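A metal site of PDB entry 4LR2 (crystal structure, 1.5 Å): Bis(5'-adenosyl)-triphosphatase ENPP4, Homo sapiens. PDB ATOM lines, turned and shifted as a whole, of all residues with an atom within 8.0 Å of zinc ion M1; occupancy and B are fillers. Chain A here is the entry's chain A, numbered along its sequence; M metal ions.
The side-chain carboxylate (OD1) of Asp 222 is in hydrogen-bond range of the backbone NH (N) of Gly 20 (3.0 Å). OG of Ser 221 sits at hydrogen-bond distance from OD1 of Asp 222 (3.2 Å). The side-chain amide oxygen (OD1) of Asn 58 sits close to the backbone carbonyl oxygen (O) of Asp 222, 3.5 Å away. ND1 of His 59 sits close to OD2 of Asp 222. A ring nitrogen (ND1) of His 59 is in hydrogen-bond range of the backbone carbonyl oxygen of Thr 55 (2.9 Å). OD2 of Asp 19 sits at hydrogen-bond distance from OH of Tyr 169 (2.7 Å). O of Asp 19 sits at hydrogen-bond distance from N of Asp 174, 2.7 Å away. O of His 223 sits at hydrogen-bond distance from N of Phe 21, at 3.2 Å.
Zinc ion M1 is bound by the side-chain hydroxyl (OG1) of Thr 55, a ring nitrogen (NE2) of His 223, the side-chain carboxylate (OD2) of Asp 222 and the side-chain carboxylate (OD1) of Asp 19. Slightly farther from zinc ion M1 lies OD2 of Asp 19 (2.8 Å).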
ATOM      1  N   SER A  17       6.014 -20.644   3.505  1.00  0.00           N
ATOM      2  CA  SER A  17       5.522 -19.390   2.932  1.00  0.00           C
ATOM      3  C   SER A  17       5.684 -18.287   3.953  1.00  0.00           C
ATOM      4  O   SER A  17       5.201 -18.419   5.096  1.00  0.00           O
ATOM      5  CB  SER A  17       4.049 -19.506   2.558  1.00  0.00           C
ATOM      6  OG  SER A  17       3.557 -18.252   2.102  1.00  0.00           O
ATOM      7  N   PHE A  18       6.386 -17.225   3.573  1.00  0.00           N
ATOM      8  CA  PHE A  18       6.339 -15.973   4.278  1.00  0.00           C
ATOM      9  C   PHE A  18       5.371 -15.052   3.543  1.00  0.00           C
ATOM     10  O   PHE A  18       5.668 -14.563   2.441  1.00  0.00           O
ATOM     11  CB  PHE A  18       7.731 -15.312   4.400  1.00  0.00           C
ATOM     12  CG  PHE A  18       8.697 -16.135   5.192  1.00  0.00           C
ATOM     13  CD1 PHE A  18       8.766 -16.011   6.576  1.00  0.00           C
ATOM     14  CD2 PHE A  18       9.549 -17.058   4.562  1.00  0.00           C
ATOM     15  CE1 PHE A  18       9.655 -16.776   7.315  1.00  0.00           C
ATOM     16  CE2 PHE A  18      10.436 -17.826   5.310  1.00  0.00           C
ATOM     17  CZ  PHE A  18      10.491 -17.682   6.677  1.00  0.00           C
ATOM     18  N   ASP A  19       4.188 -14.873   4.118  1.00  0.00           N
ATOM     19  CA  ASP A  19       3.124 -14.094   3.500  1.00  0.00           C
ATOM     20  C   ASP A  19       3.549 -12.718   2.994  1.00  0.00           C
ATOM     21  O   ASP A  19       4.202 -11.941   3.726  1.00  0.00           O
ATOM     22  CB  ASP A  19       1.953 -13.945   4.473  1.00  0.00           C
ATOM     23  CG  ASP A  19       0.651 -13.673   3.748  1.00  0.00           C
ATOM     24  OD1 ASP A  19       0.599 -12.737   2.891  1.00  0.00           O
ATOM     25  OD2 ASP A  19      -0.329 -14.382   4.027  1.00  0.00           O
ATOM     26  N   GLY A  20       3.264 -12.441   1.728  1.00  0.00           N
ATOM     27  CA  GLY A  20       3.383 -11.081   1.219  1.00  0.00           C
ATOM     28  C   GLY A  20       4.804 -10.669   0.858  1.00  0.00           C
ATOM     29  O   GLY A  20       5.173  -9.490   0.959  1.00  0.00           O
ATOM     30  N   PHE A  21       5.598 -11.648   0.435  1.00  0.00           N
ATOM     31  CA  PHE A  21       7.019 -11.425   0.123  1.00  0.00           C
ATOM     32  C   PHE A  21       7.142 -11.080  -1.376  1.00  0.00           C
ATOM     33  O   PHE A  21       7.225 -11.965  -2.243  1.00  0.00           O
ATOM     34  CB  PHE A  21       7.853 -12.649   0.516  1.00  0.00           C
ATOM     35  CG  PHE A  21       9.323 -12.352   0.667  1.00  0.00           C
ATOM     36  CD1 PHE A  21      10.029 -12.896   1.719  1.00  0.00           C
ATOM     37  CD2 PHE A  21      10.007 -11.628  -0.289  1.00  0.00           C
ATOM     38  CE1 PHE A  21      11.421 -12.651   1.872  1.00  0.00           C
ATOM     39  CE2 PHE A  21      11.374 -11.367  -0.155  1.00  0.00           C
ATOM     40  CZ  PHE A  21      12.082 -11.906   0.922  1.00  0.00           C
ATOM     41  N   THR A  53      -5.025 -11.532  -6.325  1.00  0.00           N
ATOM     42  CA  THR A  53      -3.745 -11.801  -5.688  1.00  0.00           C
ATOM     43  C   THR A  53      -3.835 -11.662  -4.159  1.00  0.00           C
ATOM     44  O   THR A  53      -3.162 -10.808  -3.536  1.00  0.00           O
ATOM     45  CB  THR A  53      -2.585 -10.970  -6.306  1.00  0.00           C
ATOM     46  OG1 THR A  53      -2.952  -9.583  -6.333  1.00  0.00           O
ATOM     47  CG2 THR A  53      -2.296 -11.412  -7.726  1.00  0.00           C
ATOM     48  N   LYS A  54      -4.699 -12.487  -3.564  1.00  0.00           N
ATOM     49  CA  LYS A  54      -4.947 -12.472  -2.122  1.00  0.00           C
ATOM     50  C   LYS A  54      -4.398 -13.755  -1.509  1.00  0.00           C
ATOM     51  O   LYS A  54      -4.061 -14.708  -2.218  1.00  0.00           O
ATOM     52  CB  LYS A  54      -6.440 -12.337  -1.851  1.00  0.00           C
ATOM     53  CG  LYS A  54      -7.029 -10.975  -2.248  1.00  0.00           C
ATOM     54  CD  LYS A  54      -6.544  -9.855  -1.360  1.00  0.00           C
ATOM     55  CE  LYS A  54      -7.462  -8.655  -1.581  1.00  0.00           C
ATOM     56  NZ  LYS A  54      -6.986  -7.412  -0.885  1.00  0.00           N
ATOM     57  N   THR A  55      -4.398 -13.802  -0.175  1.00  0.00           N
ATOM     58  CA  THR A  55      -3.714 -14.862   0.580  1.00  0.00           C
ATOM     59  C   THR A  55      -4.292 -16.263   0.478  1.00  0.00           C
ATOM     60  O   THR A  55      -3.581 -17.202   0.091  1.00  0.00           O
ATOM     61  CB  THR A  55      -3.574 -14.440   2.059  1.00  0.00           C
ATOM     62  OG1 THR A  55      -2.745 -13.260   2.124  1.00  0.00           O
ATOM     63  CG2 THR A  55      -2.977 -15.573   2.915  1.00  0.00           C
ATOM     64  N   PHE A  56      -5.557 -16.431   0.831  1.00  0.00           N
ATOM     65  CA  PHE A  56      -6.141 -17.765   0.806  1.00  0.00           C
ATOM     66  C   PHE A  56      -6.175 -18.309  -0.628  1.00  0.00           C
ATOM     67  O   PHE A  56      -5.813 -19.463  -0.850  1.00  0.00           O
ATOM     68  CB  PHE A  56      -7.500 -17.802   1.536  1.00  0.00           C
ATOM     69  CG  PHE A  56      -7.372 -17.993   3.027  1.00  0.00           C
ATOM     70  CD1 PHE A  56      -6.682 -17.072   3.805  1.00  0.00           C
ATOM     71  CD2 PHE A  56      -7.900 -19.115   3.634  1.00  0.00           C
ATOM     72  CE1 PHE A  56      -6.562 -17.243   5.174  1.00  0.00           C
ATOM     73  CE2 PHE A  56      -7.790 -19.292   5.009  1.00  0.00           C
ATOM     74  CZ  PHE A  56      -7.094 -18.355   5.783  1.00  0.00           C
ATOM     75  N   PRO A  57      -6.578 -17.490  -1.617  1.00  0.00           N
ATOM     76  CA  PRO A  57      -6.639 -18.044  -2.983  1.00  0.00           C
ATOM     77  C   PRO A  57      -5.272 -18.483  -3.500  1.00  0.00           C
ATOM     78  O   PRO A  57      -5.119 -19.590  -4.085  1.00  0.00           O
ATOM     79  CB  PRO A  57      -7.149 -16.839  -3.813  1.00  0.00           C
ATOM     80  CG  PRO A  57      -8.020 -16.093  -2.853  1.00  0.00           C
ATOM     81  CD  PRO A  57      -7.301 -16.189  -1.529  1.00  0.00           C
ATOM     82  N   ASN A  58      -4.244 -17.687  -3.248  1.00  0.00           N
ATOM     83  CA  ASN A  58      -2.923 -18.067  -3.770  1.00  0.00           C
ATOM     84  C   ASN A  58      -2.256 -19.213  -3.027  1.00  0.00           C
ATOM     85  O   ASN A  58      -1.587 -20.040  -3.669  1.00  0.00           O
ATOM     86  CB  ASN A  58      -2.002 -16.880  -3.884  1.00  0.00           C
ATOM     87  CG  ASN A  58      -2.178 -16.138  -5.202  1.00  0.00           C
ATOM     88  OD1 ASN A  58      -1.508 -16.465  -6.198  1.00  0.00           O
ATOM     89  ND2 ASN A  58      -3.101 -15.162  -5.226  1.00  0.00           N
ATOM     90  N   HIS A  59      -2.404 -19.273  -1.707  1.00  0.00           N
ATOM     91  CA  HIS A  59      -1.883 -20.450  -0.994  1.00  0.00           C
ATOM     92  C   HIS A  59      -2.539 -21.753  -1.521  1.00  0.00           C
ATOM     93  O   HIS A  59      -1.879 -22.791  -1.661  1.00  0.00           O
ATOM     94  CB  HIS A  59      -2.007 -20.341   0.540  1.00  0.00           C
ATOM     95  CG  HIS A  59      -0.969 -19.457   1.179  1.00  0.00           C
ATOM     96  ND1 HIS A  59      -1.124 -18.084   1.293  1.00  0.00           N
ATOM     97  CD2 HIS A  59       0.246 -19.738   1.708  1.00  0.00           C
ATOM     98  CE1 HIS A  59      -0.064 -17.572   1.896  1.00  0.00           C
ATOM     99  NE2 HIS A  59       0.783 -18.553   2.155  1.00  0.00           N
ATOM    100  N   ASN A  76     -10.493 -13.842   0.031  1.00  0.00           N
ATOM    101  CA  ASN A  76     -10.427 -14.038   1.469  1.00  0.00           C
ATOM    102  C   ASN A  76     -11.791 -13.944   2.139  1.00  0.00           C
ATOM    103  O   ASN A  76     -11.945 -14.411   3.257  1.00  0.00           O
ATOM    104  CB  ASN A  76      -9.431 -13.064   2.124  1.00  0.00           C
ATOM    105  CG  ASN A  76      -8.067 -13.700   2.383  1.00  0.00           C
ATOM    106  OD1 ASN A  76      -7.520 -14.405   1.513  1.00  0.00           O
ATOM    107  ND2 ASN A  76      -7.533 -13.498   3.598  1.00  0.00           N
ATOM    108  N   PRO A 122      -2.763 -22.023   5.544  1.00  0.00           N
ATOM    109  CA  PRO A 122      -4.211 -21.904   5.323  1.00  0.00           C
ATOM    110  C   PRO A 122      -4.866 -23.206   4.872  1.00  0.00           C
ATOM    111  O   PRO A 122      -4.431 -23.828   3.878  1.00  0.00           O
ATOM    112  CB  PRO A 122      -4.301 -20.848   4.226  1.00  0.00           C
ATOM    113  CG  PRO A 122      -3.131 -19.990   4.476  1.00  0.00           C
ATOM    114  CD  PRO A 122      -2.032 -20.942   4.874  1.00  0.00           C
ATOM    115  N   TYR A 169       4.055 -21.741   7.760  1.00  0.00           N
ATOM    116  CA  TYR A 169       3.520 -20.440   7.347  1.00  0.00           C
ATOM    117  C   TYR A 169       3.834 -19.354   8.372  1.00  0.00           C
ATOM    118  O   TYR A 169       3.837 -19.598   9.592  1.00  0.00           O
ATOM    119  CB  TYR A 169       2.008 -20.541   7.167  1.00  0.00           C
ATOM    120  CG  TYR A 169       1.285 -19.218   6.984  1.00  0.00           C
ATOM    121  CD1 TYR A 169       1.134 -18.657   5.732  1.00  0.00           C
ATOM    122  CD2 TYR A 169       0.747 -18.551   8.078  1.00  0.00           C
ATOM    123  CE1 TYR A 169       0.474 -17.453   5.547  1.00  0.00           C
ATOM    124  CE2 TYR A 169       0.087 -17.345   7.925  1.00  0.00           C
ATOM    125  CZ  TYR A 169      -0.049 -16.785   6.664  1.00  0.00           C
ATOM    126  OH  TYR A 169      -0.708 -15.556   6.477  1.00  0.00           O
ATOM    127  N   TRP A 170       4.092 -18.148   7.879  1.00  0.00           N
ATOM    128  CA  TRP A 170       4.368 -17.001   8.749  1.00  0.00           C
ATOM    129  C   TRP A 170       3.648 -15.792   8.172  1.00  0.00           C
ATOM    130  O   TRP A 170       3.518 -15.690   6.938  1.00  0.00           O
ATOM    131  CB  TRP A 170       5.867 -16.749   8.866  1.00  0.00           C
ATOM    132  CG  TRP A 170       6.243 -15.720   9.878  1.00  0.00           C
ATOM    133  CD1 TRP A 170       6.919 -14.565   9.646  1.00  0.00           C
ATOM    134  CD2 TRP A 170       5.990 -15.759  11.298  1.00  0.00           C
ATOM    135  NE1 TRP A 170       7.085 -13.866  10.821  1.00  0.00           N
ATOM    136  CE2 TRP A 170       6.537 -14.588  11.849  1.00  0.00           C
ATOM    137  CE3 TRP A 170       5.337 -16.665  12.139  1.00  0.00           C
ATOM    138  CZ2 TRP A 170       6.456 -14.301  13.207  1.00  0.00           C
ATOM    139  CZ3 TRP A 170       5.270 -16.380  13.487  1.00  0.00           C
ATOM    140  CH2 TRP A 170       5.826 -15.207  14.007  1.00  0.00           C
ATOM    141  N   GLU A 171       3.187 -14.891   9.039  1.00  0.00           N
ATOM    142  CA  GLU A 171       2.307 -13.795   8.646  1.00  0.00           C
ATOM    143  C   GLU A 171       3.014 -12.574   8.089  1.00  0.00           C
ATOM    144  O   GLU A 171       2.359 -11.683   7.523  1.00  0.00           O
ATOM    145  CB  GLU A 171       1.468 -13.313   9.848  1.00  0.00           C
ATOM    146  CG  GLU A 171       0.389 -14.294  10.326  1.00  0.00           C
ATOM    147  CD  GLU A 171       0.942 -15.422  11.168  1.00  0.00           C
ATOM    148  OE1 GLU A 171       0.221 -16.412  11.390  1.00  0.00           O
ATOM    149  OE2 GLU A 171       2.109 -15.321  11.615  1.00  0.00           O
ATOM    150  N   ASP A 174       3.767  -9.667   5.094  1.00  0.00           N
ATOM    151  CA  ASP A 174       2.482  -9.104   4.670  1.00  0.00           C
ATOM    152  C   ASP A 174       1.893  -8.100   5.675  1.00  0.00           C
ATOM    153  O   ASP A 174       1.545  -6.987   5.316  1.00  0.00           O
ATOM    154  CB  ASP A 174       1.489 -10.237   4.440  1.00  0.00           C
ATOM    155  CG  ASP A 174       0.169  -9.749   3.854  1.00  0.00           C
ATOM    156  OD1 ASP A 174       0.160  -9.253   2.715  1.00  0.00           O
ATOM    157  OD2 ASP A 174      -0.872  -9.883   4.516  1.00  0.00           O
ATOM    158  N   ALA A 175       1.798  -8.512   6.939  1.00  0.00           N
ATOM    159  CA  ALA A 175       1.194  -7.673   7.968  1.00  0.00           C
ATOM    160  C   ALA A 175       1.830  -6.278   8.032  1.00  0.00           C
ATOM    161  O   ALA A 175       1.112  -5.254   8.042  1.00  0.00           O
ATOM    162  CB  ALA A 175       1.279  -8.353   9.351  1.00  0.00           C
ATOM    163  N   HIS A 178       1.383  -4.021   4.859  1.00  0.00           N
ATOM    164  CA  HIS A 178       0.104  -3.297   4.880  1.00  0.00           C
ATOM    165  C   HIS A 178       0.233  -2.057   5.733  1.00  0.00           C
ATOM    166  O   HIS A 178      -0.222  -0.971   5.360  1.00  0.00           O
ATOM    167  CB  HIS A 178      -1.017  -4.166   5.457  1.00  0.00           C
ATOM    168  CG  HIS A 178      -1.560  -5.178   4.494  1.00  0.00           C
ATOM    169  ND1 HIS A 178      -2.136  -4.815   3.296  1.00  0.00           N
ATOM    170  CD2 HIS A 178      -1.607  -6.529   4.544  1.00  0.00           C
ATOM    171  CE1 HIS A 178      -2.525  -5.899   2.648  1.00  0.00           C
ATOM    172  NE2 HIS A 178      -2.209  -6.956   3.389  1.00  0.00           N
ATOM    173  N   SER A 221       6.158 -17.563  -1.435  1.00  0.00           N
ATOM    174  CA  SER A 221       5.137 -16.693  -0.878  1.00  0.00           C
ATOM    175  C   SER A 221       3.927 -16.664  -1.797  1.00  0.00           C
ATOM    176  O   SER A 221       3.907 -17.354  -2.832  1.00  0.00           O
ATOM    177  CB  SER A 221       5.667 -15.279  -0.627  1.00  0.00           C
ATOM    178  OG  SER A 221       4.709 -14.439   0.024  1.00  0.00           O
ATOM    179  N   ASP A 222       2.928 -15.894  -1.412  1.00  0.00           N
ATOM    180  CA  ASP A 222       1.665 -15.909  -2.119  1.00  0.00           C
ATOM    181  C   ASP A 222       1.459 -14.716  -3.053  1.00  0.00           C
ATOM    182  O   ASP A 222       0.719 -14.843  -4.053  1.00  0.00           O
ATOM    183  CB  ASP A 222       0.505 -16.059  -1.136  1.00  0.00           C
ATOM    184  CG  ASP A 222       0.475 -14.970  -0.048  1.00  0.00           C
ATOM    185  OD1 ASP A 222       1.503 -14.277   0.199  1.00  0.00           O
ATOM    186  OD2 ASP A 222      -0.604 -14.877   0.606  1.00  0.00           O
ATOM    187  N   HIS A 223       2.115 -13.598  -2.765  1.00  0.00           N
ATOM    188  CA  HIS A 223       1.904 -12.355  -3.521  1.00  0.00           C
ATOM    189  C   HIS A 223       2.807 -11.303  -2.935  1.00  0.00           C
ATOM    190  O   HIS A 223       3.465 -11.524  -1.921  1.00  0.00           O
ATOM    191  CB  HIS A 223       0.465 -11.822  -3.365  1.00  0.00           C
ATOM    192  CG  HIS A 223       0.048 -11.671  -1.929  1.00  0.00           C
ATOM    193  ND1 HIS A 223       0.522 -10.661  -1.114  1.00  0.00           N
ATOM    194  CD2 HIS A 223      -0.774 -12.424  -1.152  1.00  0.00           C
ATOM    195  CE1 HIS A 223       0.051 -10.825   0.115  1.00  0.00           C
ATOM    196  NE2 HIS A 223      -0.770 -11.878   0.108  1.00  0.00           N
ATOM    197  N   GLY A 224       2.829 -10.145  -3.594  1.00  0.00           N
ATOM    198  CA  GLY A 224       3.605  -9.007  -3.166  1.00  0.00           C
ATOM    199  C   GLY A 224       2.765  -7.948  -2.505  1.00  0.00           C
ATOM    200  O   GLY A 224       1.834  -8.277  -1.739  1.00  0.00           O
ATOM    201  N   MET A 225       3.089  -6.687  -2.798  1.00  0.00           N
ATOM    202  CA  MET A 225       2.499  -5.539  -2.084  1.00  0.00           C
ATOM    203  C   MET A 225       2.752  -4.303  -2.921  1.00  0.00           C
ATOM    204  O   MET A 225       3.799  -4.218  -3.567  1.00  0.00           O
ATOM    205  CB  MET A 225       3.139  -5.377  -0.709  1.00  0.00           C
ATOM    206  CG  MET A 225       2.396  -4.468   0.274  1.00  0.00           C
ATOM    207  SD  MET A 225       0.807  -5.052   0.926  1.00  0.00           S
ATOM    208  CE  MET A 225       1.363  -6.462   1.902  1.00  0.00           C
ATOM    209  N   HIS A 321      -2.534  -5.599  -1.671  1.00  0.00           N
ATOM    210  CA  HIS A 321      -2.376  -6.525  -2.779  1.00  0.00           C
ATOM    211  C   HIS A 321      -3.756  -7.028  -3.175  1.00  0.00           C
ATOM    212  O   HIS A 321      -4.775  -6.749  -2.499  1.00  0.00           O
ATOM    213  CB  HIS A 321      -1.492  -7.714  -2.377  1.00  0.00           C
ATOM    214  CG  HIS A 321      -1.906  -8.382  -1.109  1.00  0.00           C
ATOM    215  ND1 HIS A 321      -2.794  -9.437  -1.072  1.00  0.00           N
ATOM    216  CD2 HIS A 321      -1.639  -8.086   0.191  1.00  0.00           C
ATOM    217  CE1 HIS A 321      -3.022  -9.796   0.183  1.00  0.00           C
ATOM    218  NE2 HIS A 321      -2.332  -8.982   0.965  1.00  0.00           N
HETATM  219 ZN    ZN M   1      -0.909 -13.175   1.623  1.00  0.00          ZN
HETATM  220 ZN    ZN M   2      -2.384  -9.007   3.039  1.00  0.00          ZN
